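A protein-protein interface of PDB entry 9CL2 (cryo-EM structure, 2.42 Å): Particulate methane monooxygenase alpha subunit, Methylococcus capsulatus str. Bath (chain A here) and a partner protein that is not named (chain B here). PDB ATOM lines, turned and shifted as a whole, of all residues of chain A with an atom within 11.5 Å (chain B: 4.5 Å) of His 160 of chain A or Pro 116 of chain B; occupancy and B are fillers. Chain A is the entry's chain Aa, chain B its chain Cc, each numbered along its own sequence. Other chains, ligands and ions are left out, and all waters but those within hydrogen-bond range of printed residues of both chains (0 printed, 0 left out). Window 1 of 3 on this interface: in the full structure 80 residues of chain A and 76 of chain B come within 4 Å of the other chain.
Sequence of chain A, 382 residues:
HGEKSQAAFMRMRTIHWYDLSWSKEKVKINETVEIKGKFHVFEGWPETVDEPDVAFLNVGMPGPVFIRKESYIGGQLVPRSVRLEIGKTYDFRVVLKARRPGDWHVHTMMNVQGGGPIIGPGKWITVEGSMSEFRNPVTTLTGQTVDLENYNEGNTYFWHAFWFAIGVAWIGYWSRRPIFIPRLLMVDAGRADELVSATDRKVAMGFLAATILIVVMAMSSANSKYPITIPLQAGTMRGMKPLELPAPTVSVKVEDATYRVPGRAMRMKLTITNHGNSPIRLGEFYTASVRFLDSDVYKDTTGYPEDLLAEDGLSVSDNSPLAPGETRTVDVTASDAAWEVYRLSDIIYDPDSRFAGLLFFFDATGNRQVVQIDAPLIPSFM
Of the printed residues of chain B, Asn 152 of chain A touches Ile 158 (2.7 Å).
Printed residues of chain B within 4 Å of Thr 156 of chain A: Phe 115 and Ile 158.
Printed residues of chain B within 4 Å of Tyr 157 of chain A: Trp 96.
Of chain B, only Trp 96 (2.9 Å), Pro 116 (2.8 Å), Ala 117 (3.8 Å), Ser 118 (3.9 Å) and Ile 158 (3.7 Å) come within 4 Å of His 160 of chain A.
No residue of chain A comes within 4 Å of Asp 44 of chain B.
No residue of chain A comes within 4 Å of Leu 92 of chain B.
Trp 96 of chain B touches two residues of chain A.
Phe 115 of chain B touches just one residue of chain A: Thr 156 (3.8 Å).
Ala 117 of chain B touches just one residue of chain A: His 160 (3.8 Å).
Ser 118 of chain B touches just these residues of chain A: His 160 and Trp 163.
Printed residues of chain A within 4 Å of Ile 158 of chain B: Asn 152 (2.7 Å), Asn 155 (3.6 Å), Thr 156 (3.5 Å), Trp 159 (3.8 Å) and His 160 (3.7 Å).
The nearest residue of chain A that does not touch Pro 116 of chain B is Thr 156 of chain A (5.4 Å).
ND1 of His 160 of chain A is in hydrogen-bond range of NE1 of Trp 96 of chain B.
The backbone carbonyl oxygen (O) of Pro 116 of chain B is in hydrogen-bond range of a ring nitrogen (NE2) of His 160 of chain A (2.8 Å).
The side-chain amide nitrogen of Asn 152 of chain A is in hydrogen-bond range of the backbone carbonyl oxygen of Ile 158 of chain B (2.7 Å).
The side-chain carboxylate (OD1) of Asp 44 of chain B lies within hydrogen-bond range of the backbone NH (N) of Ala 117 of chain B, at 3.0 Å.
The side-chain amide nitrogen (ND2) of Asn 155 of chain A sits close to the side-chain amide oxygen (OD1) of Asn 152 of chain A, at 3.4 Å.
The backbone carbonyl oxygen of Asn 152 of chain A is in hydrogen-bond range of the side-chain hydroxyl of Thr 156 of chain A, at 2.9 Å.
OD1 of Asn 155 of chain A lies within hydrogen-bond range of NE1 of Trp 159 of chain A, 2.9 Å away.
ND2 of Asn 155 of chain A touches CA of Ile 158 of chain B, 3.6 Å away.
Thr 156 of chain A touches Phe 115 of chain B.
Thr 156 of chain A touches Ile 158 of chain B.
CE1 of Tyr 157 of chain A touches CZ3 of Trp 96 of chain B, at 3.7 Å.
Trp 159 of chain A touches Ile 158 of chain B (CB to CG1, 3.8 Å).
C of Ala 117 of chain B touches CE1 of His 160 of chain A (3.8 Å).
Ser 118 of chain B touches His 160 of chain A.
Ile 158 of chain B touches His 160 of chain A (CD1 to CD2, 3.7 Å).
Trp 163 of chain A touches Ser 118 of chain B (CD1 to OG, 3.7 Å).
Printed residues of chain B that touch a printed residue of chain A: Trp 96, Phe 115, Pro 116, Ala 117, Ser 118 and Ile 158.
Hydrophobic or aromatic side chains of chain B that line the printed part of chain A: Trp 96, Phe 115, Pro 116 and Ile 158.
Of the 20 printed residues of chain A, 7 touch a printed residue of chain B.
Hydrophobic or aromatic side chains of chain A that line the printed part of chain B: Tyr 157, Trp 159, His 160 and Trp 163.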
ATOM      1  N   ASN A 152      20.161   9.006 -34.464  1.00  0.00           N
ATOM      2  CA  ASN A 152      19.894   7.985 -33.452  1.00  0.00           C
ATOM      3  C   ASN A 152      19.973   6.563 -33.995  1.00  0.00           C
ATOM      4  O   ASN A 152      19.543   5.623 -33.315  1.00  0.00           O
ATOM      5  CB  ASN A 152      18.531   8.196 -32.779  1.00  0.00           C
ATOM      6  CG  ASN A 152      18.489   7.644 -31.371  1.00  0.00           C
ATOM      7  OD1 ASN A 152      19.489   7.662 -30.656  1.00  0.00           O
ATOM      8  ND2 ASN A 152      17.328   7.144 -30.966  1.00  0.00           N
ATOM      9  N   GLU A 153      20.510   6.372 -35.200  1.00  0.00           N
ATOM     10  CA  GLU A 153      20.614   5.031 -35.765  1.00  0.00           C
ATOM     11  C   GLU A 153      21.651   4.197 -35.019  1.00  0.00           C
ATOM     12  O   GLU A 153      21.394   3.041 -34.650  1.00  0.00           O
ATOM     13  CB  GLU A 153      20.962   5.129 -37.249  1.00  0.00           C
ATOM     14  CG  GLU A 153      20.821   3.836 -38.022  1.00  0.00           C
ATOM     15  CD  GLU A 153      21.117   4.012 -39.496  1.00  0.00           C
ATOM     16  OE1 GLU A 153      21.452   5.143 -39.903  1.00  0.00           O
ATOM     17  OE2 GLU A 153      21.016   3.021 -40.249  1.00  0.00           O
ATOM     18  N   GLY A 154      22.831   4.776 -34.780  1.00  0.00           N
ATOM     19  CA  GLY A 154      23.895   4.033 -34.129  1.00  0.00           C
ATOM     20  C   GLY A 154      23.556   3.639 -32.705  1.00  0.00           C
ATOM     21  O   GLY A 154      23.907   2.548 -32.256  1.00  0.00           O
ATOM     22  N   ASN A 155      22.870   4.522 -31.976  1.00  0.00           N
ATOM     23  CA  ASN A 155      22.473   4.203 -30.608  1.00  0.00           C
ATOM     24  C   ASN A 155      21.511   3.021 -30.575  1.00  0.00           C
ATOM     25  O   ASN A 155      21.652   2.114 -29.743  1.00  0.00           O
ATOM     26  CB  ASN A 155      21.844   5.435 -29.956  1.00  0.00           C
ATOM     27  CG  ASN A 155      21.344   5.163 -28.554  1.00  0.00           C
ATOM     28  OD1 ASN A 155      22.125   4.865 -27.653  1.00  0.00           O
ATOM     29  ND2 ASN A 155      20.035   5.270 -28.361  1.00  0.00           N
ATOM     30  N   THR A 156      20.526   3.015 -31.478  1.00  0.00           N
ATOM     31  CA  THR A 156      19.583   1.903 -31.551  1.00  0.00           C
ATOM     32  C   THR A 156      20.297   0.604 -31.899  1.00  0.00           C
ATOM     33  O   THR A 156      20.060  -0.437 -31.270  1.00  0.00           O
ATOM     34  CB  THR A 156      18.492   2.209 -32.579  1.00  0.00           C
ATOM     35  OG1 THR A 156      17.918   3.492 -32.302  1.00  0.00           O
ATOM     36  CG2 THR A 156      17.405   1.149 -32.533  1.00  0.00           C
ATOM     37  N   TYR A 157      21.181   0.648 -32.903  1.00  0.00           N
ATOM     38  CA  TYR A 157      21.946  -0.546 -33.253  1.00  0.00           C
ATOM     39  C   TYR A 157      22.759  -1.046 -32.068  1.00  0.00           C
ATOM     40  O   TYR A 157      22.766  -2.248 -31.776  1.00  0.00           O
ATOM     41  CB  TYR A 157      22.865  -0.270 -34.442  1.00  0.00           C
ATOM     42  CG  TYR A 157      22.193  -0.329 -35.794  1.00  0.00           C
ATOM     43  CD1 TYR A 157      21.314  -1.356 -36.107  1.00  0.00           C
ATOM     44  CD2 TYR A 157      22.462   0.623 -36.767  1.00  0.00           C
ATOM     45  CE1 TYR A 157      20.706  -1.423 -37.345  1.00  0.00           C
ATOM     46  CE2 TYR A 157      21.860   0.562 -38.008  1.00  0.00           C
ATOM     47  CZ  TYR A 157      20.983  -0.461 -38.292  1.00  0.00           C
ATOM     48  OH  TYR A 157      20.380  -0.523 -39.527  1.00  0.00           O
ATOM     49  N   PHE A 158      23.437  -0.136 -31.365  1.00  0.00           N
ATOM     50  CA  PHE A 158      24.287  -0.535 -30.250  1.00  0.00           C
ATOM     51  C   PHE A 158      23.477  -1.196 -29.145  1.00  0.00           C
ATOM     52  O   PHE A 158      23.849  -2.260 -28.642  1.00  0.00           O
ATOM     53  CB  PHE A 158      25.044   0.679 -29.708  1.00  0.00           C
ATOM     54  CG  PHE A 158      25.640   0.462 -28.347  1.00  0.00           C
ATOM     55  CD1 PHE A 158      26.808  -0.266 -28.195  1.00  0.00           C
ATOM     56  CD2 PHE A 158      25.034   0.989 -27.219  1.00  0.00           C
ATOM     57  CE1 PHE A 158      27.357  -0.467 -26.944  1.00  0.00           C
ATOM     58  CE2 PHE A 158      25.578   0.792 -25.966  1.00  0.00           C
ATOM     59  CZ  PHE A 158      26.741   0.063 -25.828  1.00  0.00           C
ATOM     60  N   TRP A 159      22.353  -0.584 -28.759  1.00  0.00           N
ATOM     61  CA  TRP A 159      21.582  -1.138 -27.650  1.00  0.00           C
ATOM     62  C   TRP A 159      20.944  -2.471 -28.023  1.00  0.00           C
ATOM     63  O   TRP A 159      20.953  -3.418 -27.220  1.00  0.00           O
ATOM     64  CB  TRP A 159      20.525  -0.138 -27.187  1.00  0.00           C
ATOM     65  CG  TRP A 159      21.089   0.921 -26.292  1.00  0.00           C
ATOM     66  CD1 TRP A 159      21.141   2.259 -26.540  1.00  0.00           C
ATOM     67  CD2 TRP A 159      21.706   0.725 -25.013  1.00  0.00           C
ATOM     68  NE1 TRP A 159      21.741   2.912 -25.492  1.00  0.00           N
ATOM     69  CE2 TRP A 159      22.098   1.991 -24.541  1.00  0.00           C
ATOM     70  CE3 TRP A 159      21.960  -0.398 -24.220  1.00  0.00           C
ATOM     71  CZ2 TRP A 159      22.729   2.168 -23.313  1.00  0.00           C
ATOM     72  CZ3 TRP A 159      22.588  -0.222 -23.002  1.00  0.00           C
ATOM     73  CH2 TRP A 159      22.966   1.051 -22.560  1.00  0.00           C
ATOM     74  N   HIS A 160      20.390  -2.574 -29.237  1.00  0.00           N
ATOM     75  CA  HIS A 160      19.789  -3.837 -29.645  1.00  0.00           C
ATOM     76  C   HIS A 160      20.834  -4.942 -29.740  1.00  0.00           C
ATOM     77  O   HIS A 160      20.590  -6.069 -29.294  1.00  0.00           O
ATOM     78  CB  HIS A 160      19.049  -3.669 -30.970  1.00  0.00           C
ATOM     79  CG  HIS A 160      17.630  -3.224 -30.812  1.00  0.00           C
ATOM     80  ND1 HIS A 160      16.574  -4.108 -30.768  1.00  0.00           N
ATOM     81  CD2 HIS A 160      17.091  -1.988 -30.691  1.00  0.00           C
ATOM     82  CE1 HIS A 160      15.446  -3.436 -30.624  1.00  0.00           C
ATOM     83  NE2 HIS A 160      15.731  -2.148 -30.574  1.00  0.00           N
ATOM     84  N   ALA A 161      22.008  -4.636 -30.300  1.00  0.00           N
ATOM     85  CA  ALA A 161      23.069  -5.633 -30.379  1.00  0.00           C
ATOM     86  C   ALA A 161      23.548  -6.038 -28.992  1.00  0.00           C
ATOM     87  O   ALA A 161      23.828  -7.215 -28.746  1.00  0.00           O
ATOM     88  CB  ALA A 161      24.231  -5.100 -31.215  1.00  0.00           C
ATOM     89  N   PHE A 162      23.643  -5.078 -28.070  1.00  0.00           N
ATOM     90  CA  PHE A 162      24.079  -5.378 -26.711  1.00  0.00           C
ATOM     91  C   PHE A 162      23.116  -6.340 -26.023  1.00  0.00           C
ATOM     92  O   PHE A 162      23.535  -7.349 -25.439  1.00  0.00           O
ATOM     93  CB  PHE A 162      24.209  -4.071 -25.926  1.00  0.00           C
ATOM     94  CG  PHE A 162      24.577  -4.251 -24.483  1.00  0.00           C
ATOM     95  CD1 PHE A 162      25.860  -4.622 -24.123  1.00  0.00           C
ATOM     96  CD2 PHE A 162      23.647  -4.017 -23.485  1.00  0.00           C
ATOM     97  CE1 PHE A 162      26.203  -4.777 -22.794  1.00  0.00           C
ATOM     98  CE2 PHE A 162      23.984  -4.168 -22.156  1.00  0.00           C
ATOM     99  CZ  PHE A 162      25.265  -4.548 -21.810  1.00  0.00           C
ATOM    100  N   TRP A 163      21.814  -6.055 -26.101  1.00  0.00           N
ATOM    101  CA  TRP A 163      20.852  -6.924 -25.424  1.00  0.00           C
ATOM    102  C   TRP A 163      20.745  -8.282 -26.114  1.00  0.00           C
ATOM    103  O   TRP A 163      20.598  -9.316 -25.445  1.00  0.00           O
ATOM    104  CB  TRP A 163      19.492  -6.235 -25.335  1.00  0.00           C
ATOM    105  CG  TRP A 163      19.441  -5.202 -24.244  1.00  0.00           C
ATOM    106  CD1 TRP A 163      19.189  -3.870 -24.388  1.00  0.00           C
ATOM    107  CD2 TRP A 163      19.666  -5.418 -22.843  1.00  0.00           C
ATOM    108  NE1 TRP A 163      19.235  -3.244 -23.167  1.00  0.00           N
ATOM    109  CE2 TRP A 163      19.526  -4.172 -22.202  1.00  0.00           C
ATOM    110  CE3 TRP A 163      19.966  -6.544 -22.070  1.00  0.00           C
ATOM    111  CZ2 TRP A 163      19.676  -4.019 -20.825  1.00  0.00           C
ATOM    112  CZ3 TRP A 163      20.115  -6.390 -20.703  1.00  0.00           C
ATOM    113  CH2 TRP A 163      19.971  -5.138 -20.096  1.00  0.00           C
ATOM    114  N   PHE A 164      20.836  -8.306 -27.447  1.00  0.00           N
ATOM    115  CA  PHE A 164      20.835  -9.579 -28.159  1.00  0.00           C
ATOM    116  C   PHE A 164      22.050 -10.417 -27.783  1.00  0.00           C
ATOM    117  O   PHE A 164      21.944 -11.636 -27.616  1.00  0.00           O
ATOM    118  CB  PHE A 164      20.793  -9.336 -29.667  1.00  0.00           C
ATOM    119  CG  PHE A 164      20.215 -10.481 -30.449  1.00  0.00           C
ATOM    120  CD1 PHE A 164      21.016 -11.536 -30.853  1.00  0.00           C
ATOM    121  CD2 PHE A 164      18.871 -10.503 -30.779  1.00  0.00           C
ATOM    122  CE1 PHE A 164      20.487 -12.590 -31.572  1.00  0.00           C
ATOM    123  CE2 PHE A 164      18.336 -11.553 -31.498  1.00  0.00           C
ATOM    124  CZ  PHE A 164      19.145 -12.598 -31.894  1.00  0.00           C
ATOM    125  N   ALA A 165      23.214  -9.778 -27.644  1.00  0.00           N
ATOM    126  CA  ALA A 165      24.414 -10.494 -27.231  1.00  0.00           C
ATOM    127  C   ALA A 165      24.275 -11.031 -25.814  1.00  0.00           C
ATOM    128  O   ALA A 165      24.735 -12.138 -25.517  1.00  0.00           O
ATOM    129  CB  ALA A 165      25.635  -9.582 -27.342  1.00  0.00           C
ATOM    130  N   ILE A 166      23.653 -10.259 -24.919  1.00  0.00           N
ATOM    131  CA  ILE A 166      23.430 -10.750 -23.561  1.00  0.00           C
ATOM    132  C   ILE A 166      22.536 -11.986 -23.577  1.00  0.00           C
ATOM    133  O   ILE A 166      22.819 -12.986 -22.904  1.00  0.00           O
ATOM    134  CB  ILE A 166      22.846  -9.637 -22.672  1.00  0.00           C
ATOM    135  CG1 ILE A 166      23.948  -8.675 -22.234  1.00  0.00           C
ATOM    136  CG2 ILE A 166      22.146 -10.228 -21.455  1.00  0.00           C
ATOM    137  CD1 ILE A 166      23.448  -7.531 -21.394  1.00  0.00           C
ATOM    138  N   GLY A 167      21.449 -11.941 -24.351  1.00  0.00           N
ATOM    139  CA  GLY A 167      20.582 -13.108 -24.450  1.00  0.00           C
ATOM    140  C   GLY A 167      21.281 -14.312 -25.056  1.00  0.00           C
ATOM    141  O   GLY A 167      21.107 -15.448 -24.595  1.00  0.00           O
ATOM    142  N   VAL A 168      22.086 -14.080 -26.095  1.00  0.00           N
ATOM    143  CA  VAL A 168      22.825 -15.165 -26.734  1.00  0.00           C
ATOM    144  C   VAL A 168      23.819 -15.778 -25.758  1.00  0.00           C
ATOM    145  O   VAL A 168      23.991 -17.000 -25.715  1.00  0.00           O
ATOM    146  CB  VAL A 168      23.518 -14.658 -28.013  1.00  0.00           C
ATOM    147  CG1 VAL A 168      24.577 -15.643 -28.480  1.00  0.00           C
ATOM    148  CG2 VAL A 168      22.492 -14.428 -29.110  1.00  0.00           C
ATOM    149  N   ALA A 169      24.495 -14.943 -24.965  1.00  0.00           N
ATOM    150  CA  ALA A 169      25.419 -15.458 -23.960  1.00  0.00           C
ATOM    151  C   ALA A 169      24.686 -16.275 -22.904  1.00  0.00           C
ATOM    152  O   ALA A 169      25.176 -17.326 -22.471  1.00  0.00           O
ATOM    153  CB  ALA A 169      26.185 -14.306 -23.312  1.00  0.00           C
ATOM    154  N   ILE A 214      22.167  -2.688 -15.058  1.00  0.00           N
ATOM    155  CA  ILE A 214      22.466  -2.093 -16.354  1.00  0.00           C
ATOM    156  C   ILE A 214      21.275  -1.296 -16.862  1.00  0.00           C
ATOM    157  O   ILE A 214      21.440  -0.201 -17.409  1.00  0.00           O
ATOM    158  CB  ILE A 214      22.895  -3.182 -17.355  1.00  0.00           C
ATOM    159  CG1 ILE A 214      24.334  -3.622 -17.082  1.00  0.00           C
ATOM    160  CG2 ILE A 214      22.754  -2.689 -18.788  1.00  0.00           C
ATOM    161  CD1 ILE A 214      24.740  -4.869 -17.833  1.00  0.00           C
ATOM    162  N   ALA A 218      21.558   2.652 -17.497  1.00  0.00           N
ATOM    163  CA  ALA A 218      21.290   3.154 -18.837  1.00  0.00           C
ATOM    164  C   ALA A 218      20.183   4.199 -18.823  1.00  0.00           C
ATOM    165  O   ALA A 218      20.276   5.214 -19.520  1.00  0.00           O
ATOM    166  CB  ALA A 218      20.928   1.998 -19.767  1.00  0.00           C
ATOM    167  N   ASP B  44       5.046  -1.327 -32.633  1.00  0.00           N
ATOM    168  CA  ASP B  44       6.424  -1.760 -32.832  1.00  0.00           C
ATOM    169  C   ASP B  44       7.013  -1.283 -34.153  1.00  0.00           C
ATOM    170  O   ASP B  44       8.239  -1.177 -34.265  1.00  0.00           O
ATOM    171  CB  ASP B  44       6.501  -3.288 -32.757  1.00  0.00           C
ATOM    172  CG  ASP B  44       7.928  -3.801 -32.735  1.00  0.00           C
ATOM    173  OD1 ASP B  44       8.608  -3.626 -31.702  1.00  0.00           O
ATOM    174  OD2 ASP B  44       8.369  -4.378 -33.750  1.00  0.00           O
ATOM    175  N   LEU B  92      12.961 -11.021 -31.852  1.00  0.00           N
ATOM    176  CA  LEU B  92      13.812  -9.899 -32.227  1.00  0.00           C
ATOM    177  C   LEU B  92      14.532 -10.164 -33.541  1.00  0.00           C
ATOM    178  O   LEU B  92      14.662  -9.263 -34.376  1.00  0.00           O
ATOM    179  CB  LEU B  92      14.819  -9.608 -31.113  1.00  0.00           C
ATOM    180  CG  LEU B  92      14.276  -8.848 -29.904  1.00  0.00           C
ATOM    181  CD1 LEU B  92      15.251  -8.928 -28.745  1.00  0.00           C
ATOM    182  CD2 LEU B  92      13.987  -7.402 -30.269  1.00  0.00           C
ATOM    183  N   GLU B  95      11.966  -9.794 -36.381  1.00  0.00           N
ATOM    184  CA  GLU B  95      11.592  -8.395 -36.547  1.00  0.00           C
ATOM    185  C   GLU B  95      12.712  -7.596 -37.199  1.00  0.00           C
ATOM    186  O   GLU B  95      12.462  -6.814 -38.120  1.00  0.00           O
ATOM    187  CB  GLU B  95      11.214  -7.789 -35.196  1.00  0.00           C
ATOM    188  CG  GLU B  95       9.781  -8.067 -34.775  1.00  0.00           C
ATOM    189  CD  GLU B  95       9.498  -7.637 -33.351  1.00  0.00           C
ATOM    190  OE1 GLU B  95       8.335  -7.752 -32.916  1.00  0.00           O
ATOM    191  OE2 GLU B  95      10.442  -7.193 -32.665  1.00  0.00           O
ATOM    192  N   TRP B  96      13.954  -7.786 -36.746  1.00  0.00           N
ATOM    193  CA  TRP B  96      15.068  -7.036 -37.313  1.00  0.00           C
ATOM    194  C   TRP B  96      15.322  -7.422 -38.763  1.00  0.00           C
ATOM    195  O   TRP B  96      15.641  -6.559 -39.591  1.00  0.00           O
ATOM    196  CB  TRP B  96      16.327  -7.243 -36.474  1.00  0.00           C
ATOM    197  CG  TRP B  96      16.542  -6.162 -35.468  1.00  0.00           C
ATOM    198  CD1 TRP B  96      16.494  -6.283 -34.111  1.00  0.00           C
ATOM    199  CD2 TRP B  96      16.826  -4.784 -35.738  1.00  0.00           C
ATOM    200  NE1 TRP B  96      16.738  -5.068 -33.519  1.00  0.00           N
ATOM    201  CE2 TRP B  96      16.945  -4.131 -34.496  1.00  0.00           C
ATOM    202  CE3 TRP B  96      16.997  -4.041 -36.909  1.00  0.00           C
ATOM    203  CZ2 TRP B  96      17.223  -2.770 -34.393  1.00  0.00           C
ATOM    204  CZ3 TRP B  96      17.272  -2.691 -36.805  1.00  0.00           C
ATOM    205  CH2 TRP B  96      17.384  -2.070 -35.556  1.00  0.00           C
ATOM    206  N   ARG B  99      12.703  -5.580 -40.713  1.00  0.00           N
ATOM    207  CA  ARG B  99      12.944  -4.139 -40.762  1.00  0.00           C
ATOM    208  C   ARG B  99      14.076  -3.800 -41.722  1.00  0.00           C
ATOM    209  O   ARG B  99      13.971  -2.849 -42.506  1.00  0.00           O
ATOM    210  CB  ARG B  99      13.263  -3.584 -39.371  1.00  0.00           C
ATOM    211  CG  ARG B  99      12.237  -3.867 -38.290  1.00  0.00           C
ATOM    212  CD  ARG B  99      10.821  -3.603 -38.754  1.00  0.00           C
ATOM    213  NE  ARG B  99       9.847  -4.317 -37.938  1.00  0.00           N
ATOM    214  CZ  ARG B  99       9.420  -3.912 -36.751  1.00  0.00           C
ATOM    215  NH1 ARG B  99       9.855  -2.787 -36.206  1.00  0.00           N
ATOM    216  NH2 ARG B  99       8.534  -4.652 -36.092  1.00  0.00           N
ATOM    217  N   PHE B 115      12.192   0.618 -36.004  1.00  0.00           N
ATOM    218  CA  PHE B 115      13.014  -0.289 -35.220  1.00  0.00           C
ATOM    219  C   PHE B 115      12.144  -0.966 -34.172  1.00  0.00           C
ATOM    220  O   PHE B 115      11.172  -0.372 -33.691  1.00  0.00           O
ATOM    221  CB  PHE B 115      14.187   0.438 -34.537  1.00  0.00           C
ATOM    222  CG  PHE B 115      13.768   1.565 -33.635  1.00  0.00           C
ATOM    223  CD1 PHE B 115      13.500   1.335 -32.296  1.00  0.00           C
ATOM    224  CD2 PHE B 115      13.660   2.857 -34.121  1.00  0.00           C
ATOM    225  CE1 PHE B 115      13.119   2.368 -31.463  1.00  0.00           C
ATOM    226  CE2 PHE B 115      13.279   3.893 -33.292  1.00  0.00           C
ATOM    227  CZ  PHE B 115      13.009   3.648 -31.962  1.00  0.00           C
ATOM    228  N   PRO B 116      12.462  -2.203 -33.806  1.00  0.00           N
ATOM    229  CA  PRO B 116      11.680  -2.900 -32.782  1.00  0.00           C
ATOM    230  C   PRO B 116      12.062  -2.438 -31.381  1.00  0.00           C
ATOM    231  O   PRO B 116      13.030  -1.706 -31.172  1.00  0.00           O
ATOM    232  CB  PRO B 116      12.033  -4.376 -32.991  1.00  0.00           C
ATOM    233  CG  PRO B 116      13.301  -4.387 -33.764  1.00  0.00           C
ATOM    234  CD  PRO B 116      13.512  -3.049 -34.400  1.00  0.00           C
ATOM    235  N   ALA B 117      11.265  -2.877 -30.413  1.00  0.00           N
ATOM    236  CA  ALA B 117      11.496  -2.566 -29.013  1.00  0.00           C
ATOM    237  C   ALA B 117      12.359  -3.638 -28.358  1.00  0.00           C
ATOM    238  O   ALA B 117      12.281  -4.821 -28.699  1.00  0.00           O
ATOM    239  CB  ALA B 117      10.171  -2.437 -28.261  1.00  0.00           C
ATOM    240  N   SER B 118      13.189  -3.208 -27.410  1.00  0.00           N
ATOM    241  CA  SER B 118      14.031  -4.142 -26.676  1.00  0.00           C
ATOM    242  C   SER B 118      13.193  -4.971 -25.710  1.00  0.00           C
ATOM    243  O   SER B 118      12.313  -4.450 -25.019  1.00  0.00           O
ATOM    244  CB  SER B 118      15.122  -3.390 -25.916  1.00  0.00           C
ATOM    245  OG  SER B 118      16.319  -3.327 -26.672  1.00  0.00           O
ATOM    246  N   ILE B 158      16.900   4.052 -25.908  1.00  0.00           N
ATOM    247  CA  ILE B 158      16.778   4.073 -27.362  1.00  0.00           C
ATOM    248  C   ILE B 158      15.885   5.220 -27.821  1.00  0.00           C
ATOM    249  O   ILE B 158      16.219   5.940 -28.767  1.00  0.00           O
ATOM    250  CB  ILE B 158      16.260   2.716 -27.868  1.00  0.00           C
ATOM    251  CG1 ILE B 158      17.191   1.588 -27.417  1.00  0.00           C
ATOM    252  CG2 ILE B 158      16.124   2.725 -29.380  1.00  0.00           C
ATOM    253  CD1 ILE B 158      16.646   0.205 -27.689  1.00  0.00           C
